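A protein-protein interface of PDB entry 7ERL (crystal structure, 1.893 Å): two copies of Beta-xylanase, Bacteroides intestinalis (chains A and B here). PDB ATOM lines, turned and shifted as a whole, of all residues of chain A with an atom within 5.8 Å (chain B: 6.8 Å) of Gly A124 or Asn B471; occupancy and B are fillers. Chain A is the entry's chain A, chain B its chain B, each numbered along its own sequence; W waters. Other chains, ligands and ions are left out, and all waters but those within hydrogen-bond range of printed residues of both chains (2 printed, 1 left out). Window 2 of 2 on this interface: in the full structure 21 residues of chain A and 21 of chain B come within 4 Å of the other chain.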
ATOM      1  N   THR A 116     -26.954  11.977  18.885  1.00  0.00           N
ATOM      2  CA  THR A 116     -26.225  12.295  20.111  1.00  0.00           C
ATOM      3  C   THR A 116     -24.962  13.067  19.751  1.00  0.00           C
ATOM      4  O   THR A 116     -24.715  13.386  18.585  1.00  0.00           O
ATOM      5  CB  THR A 116     -25.917  11.022  20.915  1.00  0.00           C
ATOM      6  OG1 THR A 116     -25.463  11.373  22.237  1.00  0.00           O
ATOM      7  CG2 THR A 116     -24.851  10.163  20.222  1.00  0.00           C
ATOM      8  N   THR A 117     -24.180  13.407  20.777  1.00  0.00           N
ATOM      9  CA  THR A 117     -22.868  14.012  20.598  1.00  0.00           C
ATOM     10  C   THR A 117     -21.836  13.090  21.224  1.00  0.00           C
ATOM     11  O   THR A 117     -21.969  12.726  22.399  1.00  0.00           O
ATOM     12  CB  THR A 117     -22.767  15.404  21.248  1.00  0.00           C
ATOM     13  OG1 THR A 117     -23.981  16.146  21.039  1.00  0.00           O
ATOM     14  CG2 THR A 117     -21.592  16.157  20.660  1.00  0.00           C
ATOM     15  N   GLN A 118     -20.823  12.701  20.442  1.00  0.00           N
ATOM     16  CA  GLN A 118     -19.737  11.855  20.938  1.00  0.00           C
ATOM     17  C   GLN A 118     -18.431  12.629  20.828  1.00  0.00           C
ATOM     18  O   GLN A 118     -17.916  12.849  19.723  1.00  0.00           O
ATOM     19  CB  GLN A 118     -19.635  10.518  20.192  1.00  0.00           C
ATOM     20  CG  GLN A 118     -18.501   9.639  20.789  1.00  0.00           C
ATOM     21  CD  GLN A 118     -18.413   8.225  20.224  1.00  0.00           C
ATOM     22  OE1 GLN A 118     -17.388   7.573  20.374  1.00  0.00           O
ATOM     23  NE2 GLN A 118     -19.488   7.741  19.587  1.00  0.00           N
ATOM     24  N   PHE A 119     -17.893  13.030  21.976  1.00  0.00           N
ATOM     25  CA  PHE A 119     -16.613  13.736  22.021  1.00  0.00           C
ATOM     26  C   PHE A 119     -15.491  12.706  22.072  1.00  0.00           C
ATOM     27  O   PHE A 119     -14.851  12.473  23.103  1.00  0.00           O
ATOM     28  CB  PHE A 119     -16.565  14.686  23.209  1.00  0.00           C
ATOM     29  CG  PHE A 119     -17.479  15.855  23.078  1.00  0.00           C
ATOM     30  CD1 PHE A 119     -17.125  16.947  22.298  1.00  0.00           C
ATOM     31  CD2 PHE A 119     -18.697  15.875  23.740  1.00  0.00           C
ATOM     32  CE1 PHE A 119     -17.979  18.045  22.173  1.00  0.00           C
ATOM     33  CE2 PHE A 119     -19.542  16.968  23.631  1.00  0.00           C
ATOM     34  CZ  PHE A 119     -19.182  18.055  22.836  1.00  0.00           C
ATOM     35  N   ALA A 120     -15.268  12.082  20.908  1.00  0.00           N
ATOM     36  CA  ALA A 120     -14.306  11.001  20.730  1.00  0.00           C
ATOM     37  C   ALA A 120     -14.356  10.541  19.283  1.00  0.00           C
ATOM     38  O   ALA A 120     -15.404  10.650  18.646  1.00  0.00           O
ATOM     39  CB  ALA A 120     -14.610   9.821  21.663  1.00  0.00           C
ATOM     40  N   GLY A 121     -13.237  10.051  18.753  1.00  0.00           N
ATOM     41  CA  GLY A 121     -13.225   9.437  17.432  1.00  0.00           C
ATOM     42  C   GLY A 121     -13.515  10.377  16.287  1.00  0.00           C
ATOM     43  O   GLY A 121     -13.813   9.919  15.177  1.00  0.00           O
ATOM     44  N   GLY A 122     -13.434  11.686  16.518  1.00  0.00           N
ATOM     45  CA  GLY A 122     -13.811  12.637  15.491  1.00  0.00           C
ATOM     46  C   GLY A 122     -15.293  12.721  15.186  1.00  0.00           C
ATOM     47  O   GLY A 122     -15.665  13.362  14.200  1.00  0.00           O
ATOM     48  N   PHE A 123     -16.155  12.118  16.015  1.00  0.00           N
ATOM     49  CA  PHE A 123     -17.575  11.999  15.682  1.00  0.00           C
ATOM     50  C   PHE A 123     -18.330  13.311  15.858  1.00  0.00           C
ATOM     51  O   PHE A 123     -19.054  13.743  14.953  1.00  0.00           O
ATOM     52  CB  PHE A 123     -18.227  10.912  16.539  1.00  0.00           C
ATOM     53  CG  PHE A 123     -17.956   9.505  16.054  1.00  0.00           C
ATOM     54  CD1 PHE A 123     -18.281   9.125  14.761  1.00  0.00           C
ATOM     55  CD2 PHE A 123     -17.370   8.567  16.897  1.00  0.00           C
ATOM     56  CE1 PHE A 123     -18.034   7.822  14.303  1.00  0.00           C
ATOM     57  CE2 PHE A 123     -17.115   7.264  16.458  1.00  0.00           C
ATOM     58  CZ  PHE A 123     -17.450   6.891  15.153  1.00  0.00           C
ATOM     59  N   GLY A 124     -18.223  13.933  17.032  1.00  0.00           N
ATOM     60  CA  GLY A 124     -19.089  15.072  17.289  1.00  0.00           C
ATOM     61  C   GLY A 124     -20.548  14.655  17.254  1.00  0.00           C
ATOM     62  O   GLY A 124     -20.925  13.566  17.704  1.00  0.00           O
ATOM     63  N   ASN A 125     -21.384  15.522  16.703  1.00  0.00           N
ATOM     64  CA  ASN A 125     -22.797  15.203  16.584  1.00  0.00           C
ATOM     65  C   ASN A 125     -23.019  14.149  15.503  1.00  0.00           C
ATOM     66  O   ASN A 125     -22.542  14.291  14.372  1.00  0.00           O
ATOM     67  CB  ASN A 125     -23.588  16.467  16.288  1.00  0.00           C
ATOM     68  CG  ASN A 125     -23.785  17.293  17.524  1.00  0.00           C
ATOM     69  OD1 ASN A 125     -24.401  16.831  18.473  1.00  0.00           O
ATOM     70  ND2 ASN A 125     -23.230  18.504  17.543  1.00  0.00           N
ATOM     71  N   ILE A 126     -23.731  13.080  15.876  1.00  0.00           N
ATOM     72  CA  ILE A 126     -23.891  11.894  15.042  1.00  0.00           C
ATOM     73  C   ILE A 126     -25.315  11.396  15.184  1.00  0.00           C
ATOM     74  O   ILE A 126     -26.011  11.693  16.158  1.00  0.00           O
ATOM     75  CB  ILE A 126     -22.919  10.759  15.427  1.00  0.00           C
ATOM     76  CG1 ILE A 126     -22.933  10.565  16.957  1.00  0.00           C
ATOM     77  CG2 ILE A 126     -21.520  11.042  14.897  1.00  0.00           C
ATOM     78  CD1 ILE A 126     -22.271   9.262  17.436  1.00  0.00           C
ATOM     79  N   LYS A 142     -22.068  11.367  10.631  1.00  0.00           N
ATOM     80  CA  LYS A 142     -21.675  12.642  11.221  1.00  0.00           C
ATOM     81  C   LYS A 142     -22.543  13.785  10.698  1.00  0.00           C
ATOM     82  O   LYS A 142     -22.760  13.911   9.488  1.00  0.00           O
ATOM     83  CB  LYS A 142     -20.199  12.915  10.931  1.00  0.00           C
ATOM     84  CG  LYS A 142     -19.279  12.036  11.774  1.00  0.00           C
ATOM     85  CD  LYS A 142     -17.884  11.943  11.203  1.00  0.00           C
ATOM     86  CE  LYS A 142     -17.139  13.237  11.375  1.00  0.00           C
ATOM     87  NZ  LYS A 142     -15.672  13.003  11.231  1.00  0.00           N
ATOM     88  N   LYS B 403      -3.655  12.993  21.331  1.00  0.00           N
ATOM     89  CA  LYS B 403      -4.811  12.904  22.219  1.00  0.00           C
ATOM     90  C   LYS B 403      -4.585  12.012  23.439  1.00  0.00           C
ATOM     91  O   LYS B 403      -5.411  12.033  24.365  1.00  0.00           O
ATOM     92  CB  LYS B 403      -6.030  12.389  21.448  1.00  0.00           C
ATOM     93  CG  LYS B 403      -6.753  13.467  20.663  1.00  0.00           C
ATOM     94  CD  LYS B 403      -8.037  12.908  20.033  1.00  0.00           C
ATOM     95  CE  LYS B 403      -7.707  11.856  18.991  1.00  0.00           C
ATOM     96  NZ  LYS B 403      -6.835  12.430  17.909  1.00  0.00           N
ATOM     97  N   GLU B 445      -3.961  17.425  25.853  1.00  0.00           N
ATOM     98  CA  GLU B 445      -4.298  16.401  24.877  1.00  0.00           C
ATOM     99  C   GLU B 445      -5.724  16.557  24.358  1.00  0.00           C
ATOM    100  O   GLU B 445      -6.039  16.037  23.282  1.00  0.00           O
ATOM    101  CB  GLU B 445      -4.098  15.016  25.501  1.00  0.00           C
ATOM    102  CG  GLU B 445      -5.124  14.677  26.591  1.00  0.00           C
ATOM    103  CD  GLU B 445      -4.785  15.251  27.962  1.00  0.00           C
ATOM    104  OE1 GLU B 445      -3.771  15.982  28.107  1.00  0.00           O
ATOM    105  OE2 GLU B 445      -5.544  14.966  28.910  1.00  0.00           O
ATOM    106  N   ASN B 446      -6.591  17.267  25.093  1.00  0.00           N
ATOM    107  CA  ASN B 446      -7.997  17.441  24.724  1.00  0.00           C
ATOM    108  C   ASN B 446      -8.287  18.768  24.039  1.00  0.00           C
ATOM    109  O   ASN B 446      -9.394  18.941  23.515  1.00  0.00           O
ATOM    110  CB  ASN B 446      -8.889  17.311  25.969  1.00  0.00           C
ATOM    111  CG  ASN B 446      -8.884  15.905  26.539  1.00  0.00           C
ATOM    112  OD1 ASN B 446      -9.111  14.941  25.816  1.00  0.00           O
ATOM    113  ND2 ASN B 446      -8.615  15.782  27.830  1.00  0.00           N
ATOM    114  N   LYS B 466      -8.223  20.330  14.593  1.00  0.00           N
ATOM    115  CA  LYS B 466      -8.553  20.945  15.872  1.00  0.00           C
ATOM    116  C   LYS B 466      -9.091  19.866  16.805  1.00  0.00           C
ATOM    117  O   LYS B 466      -9.972  19.094  16.413  1.00  0.00           O
ATOM    118  CB  LYS B 466      -9.587  22.067  15.683  1.00  0.00           C
ATOM    119  CG  LYS B 466     -10.262  22.564  16.956  1.00  0.00           C
ATOM    120  CD  LYS B 466     -11.313  23.644  16.654  1.00  0.00           C
ATOM    121  CE  LYS B 466     -12.128  24.023  17.898  1.00  0.00           C
ATOM    122  NZ  LYS B 466     -13.209  25.021  17.582  1.00  0.00           N
ATOM    123  N   THR B 467      -8.545  19.795  18.021  1.00  0.00           N
ATOM    124  CA  THR B 467      -9.031  18.880  19.047  1.00  0.00           C
ATOM    125  C   THR B 467      -9.690  19.705  20.139  1.00  0.00           C
ATOM    126  O   THR B 467      -9.066  20.611  20.697  1.00  0.00           O
ATOM    127  CB  THR B 467      -7.904  18.022  19.628  1.00  0.00           C
ATOM    128  OG1 THR B 467      -7.224  17.355  18.565  1.00  0.00           O
ATOM    129  CG2 THR B 467      -8.467  16.950  20.589  1.00  0.00           C
ATOM    130  N   GLU B 468     -10.943  19.392  20.438  1.00  0.00           N
ATOM    131  CA  GLU B 468     -11.711  20.101  21.451  1.00  0.00           C
ATOM    132  C   GLU B 468     -12.461  19.061  22.267  1.00  0.00           C
ATOM    133  O   GLU B 468     -13.170  18.228  21.695  1.00  0.00           O
ATOM    134  CB  GLU B 468     -12.682  21.094  20.805  1.00  0.00           C
ATOM    135  CG  GLU B 468     -13.443  21.942  21.810  1.00  0.00           C
ATOM    136  CD  GLU B 468     -14.454  22.860  21.147  1.00  0.00           C
ATOM    137  OE1 GLU B 468     -15.585  22.400  20.875  1.00  0.00           O
ATOM    138  OE2 GLU B 468     -14.108  24.028  20.872  1.00  0.00           O
ATOM    139  N   LYS B 469     -12.276  19.074  23.589  1.00  0.00           N
ATOM    140  CA  LYS B 469     -12.840  18.029  24.449  1.00  0.00           C
ATOM    141  C   LYS B 469     -12.417  16.631  23.998  1.00  0.00           C
ATOM    142  O   LYS B 469     -13.184  15.668  24.101  1.00  0.00           O
ATOM    143  CB  LYS B 469     -14.363  18.136  24.516  1.00  0.00           C
ATOM    144  CG  LYS B 469     -14.830  19.354  25.268  1.00  0.00           C
ATOM    145  CD  LYS B 469     -16.285  19.635  25.007  1.00  0.00           C
ATOM    146  CE  LYS B 469     -17.146  18.711  25.831  1.00  0.00           C
ATOM    147  NZ  LYS B 469     -17.368  19.272  27.196  1.00  0.00           N
ATOM    148  N   GLY B 470     -11.178  16.503  23.513  1.00  0.00           N
ATOM    149  CA  GLY B 470     -10.671  15.207  23.092  1.00  0.00           C
ATOM    150  C   GLY B 470     -11.209  14.703  21.766  1.00  0.00           C
ATOM    151  O   GLY B 470     -10.987  13.531  21.427  1.00  0.00           O
ATOM    152  N   ASN B 471     -11.905  15.548  21.010  1.00  0.00           N
ATOM    153  CA  ASN B 471     -12.474  15.199  19.712  1.00  0.00           C
ATOM    154  C   ASN B 471     -11.746  15.964  18.607  1.00  0.00           C
ATOM    155  O   ASN B 471     -11.809  17.197  18.560  1.00  0.00           O
ATOM    156  CB  ASN B 471     -13.964  15.522  19.683  1.00  0.00           C
ATOM    157  CG  ASN B 471     -14.680  14.853  18.534  1.00  0.00           C
ATOM    158  OD1 ASN B 471     -14.451  13.677  18.256  1.00  0.00           O
ATOM    159  ND2 ASN B 471     -15.557  15.602  17.855  1.00  0.00           N
ATOM    160  N   THR B 472     -11.092  15.239  17.707  1.00  0.00           N
ATOM    161  CA  THR B 472     -10.292  15.837  16.638  1.00  0.00           C
ATOM    162  C   THR B 472     -11.118  15.956  15.362  1.00  0.00           C
ATOM    163  O   THR B 472     -11.706  14.971  14.908  1.00  0.00           O
ATOM    164  CB  THR B 472      -9.037  15.003  16.371  1.00  0.00           C
ATOM    165  OG1 THR B 472      -8.198  15.005  17.538  1.00  0.00           O
ATOM    166  CG2 THR B 472      -8.246  15.592  15.187  1.00  0.00           C
ATOM    167  N   ARG B 473     -11.172  17.161  14.796  1.00  0.00           N
ATOM    168  CA  ARG B 473     -11.842  17.418  13.528  1.00  0.00           C
ATOM    169  C   ARG B 473     -10.844  18.047  12.562  1.00  0.00           C
ATOM    170  O   ARG B 473     -10.042  18.903  12.952  1.00  0.00           O
ATOM    171  CB  ARG B 473     -13.049  18.354  13.694  1.00  0.00           C
ATOM    172  CG  ARG B 473     -14.151  17.899  14.682  1.00  0.00           C
ATOM    173  CD  ARG B 473     -14.770  16.548  14.314  1.00  0.00           C
ATOM    174  NE  ARG B 473     -15.420  16.529  13.001  1.00  0.00           N
ATOM    175  CZ  ARG B 473     -16.729  16.680  12.797  1.00  0.00           C
ATOM    176  NH1 ARG B 473     -17.549  16.873  13.818  1.00  0.00           N
ATOM    177  NH2 ARG B 473     -17.220  16.636  11.562  1.00  0.00           N
HETATM  178  O   HOH W   1     -20.154  15.907  13.239  1.00  0.00           O
HETATM  179  O   HOH W   2     -12.253  11.671  23.568  1.00  0.00           O
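The side-chain amide oxygen (OD1) of Asn B471 lies close to the backbone carbonyl oxygen (O) of Ala A120, at 3.2 Å.
N of Gly A122 is in hydrogen-bond range of OD1 of Asn B471 (2.8 Å).
The backbone carbonyl oxygen (O) of Gly A122 sits close to the guanidinium group (NE) of Arg B473 (3.4 Å).
OD1 of Asn B471 is in hydrogen-bond range of N of Phe A123 (3.2 Å).
The backbone NH (N) of Gly A124 lies close to the side-chain amide nitrogen (ND2) of Asn B471, 3.3 Å away.
The backbone NH of Gln A118 sits at hydrogen-bond distance from the backbone carbonyl oxygen of Gly A124.
The side-chain amino group (NZ) of Lys A142 is in hydrogen-bond range of the backbone carbonyl oxygen (O) of Gly A122.
OG1 of Thr B472 is in hydrogen-bond range of NZ of Lys B403 (2.9 Å).
The backbone carbonyl oxygen of Asn B446 is in hydrogen-bond range of the backbone NH of Lys B469 (2.9 Å).
The backbone carbonyl oxygen of Lys B466 sits at hydrogen-bond distance from the backbone NH of Arg B473 (2.8 Å).
OG1 of Thr B467 lies within hydrogen-bond range of OG1 of Thr B472 (2.7 Å).
O of Gln A118 touches OD1 of Asn B471, 3.9 Å away.
O of Lys B469 touches CB of Phe A119, at 3.6 Å.
CA of Phe A119 touches CB of Asn B471, 3.96 Å away.
Gly A121 touches Asn B471 (N to OD1, 3.9 Å).
Thr B472 touches Gly A122.
O of Phe A123 touches NH1 of Arg B473 (3.7 Å).
Lys A142 touches Arg B473 (CE to NH2, 3.4 Å).
Of the printed residues of chain B, Gly A122 touches Asn B471, Thr B472 and Arg B473.
Of the printed residues of chain A, Arg B473 touches Gly A122, Phe A123 and Lys A142.
Of the printed residues of chain B, Gly A121 touches Asn B471.
Of the printed residues of chain B, Phe A119 touches Lys B469 and Asn B471.
Of the printed residues of chain B, Phe A123 touches Asn B471 (3.2 Å) and Arg B473 (3.7 Å).
The nearest residue of chain B that does not touch Gly A124 is Arg B473 (4.2 Å).
Of the 12 printed residues of chain A, 8 touch a printed residue of chain B.
Hydrophobic or aromatic side chains of chain A within 4 Å of the printed part of chain B: Phe A119.
Among the printed residues, 12 pairs touch across the chains.
Among the printed residues, no Asp or Glu carboxylate lies within 4 Å of a Lys or Arg side-chain nitrogen of the other chain.
No position is printed for both chains.
Water W2 lies within hydrogen-bond range of the backbone carbonyl oxygen of Phe A119 (2.8 Å) and the backbone carbonyl oxygen of Gly B470 (3.1 Å).
Water W1 lies within hydrogen-bond range of NH1 of Arg B473 (2.8 Å), O of Phe A123 (3.0 Å) and O of Asn A125 (3.1 Å).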
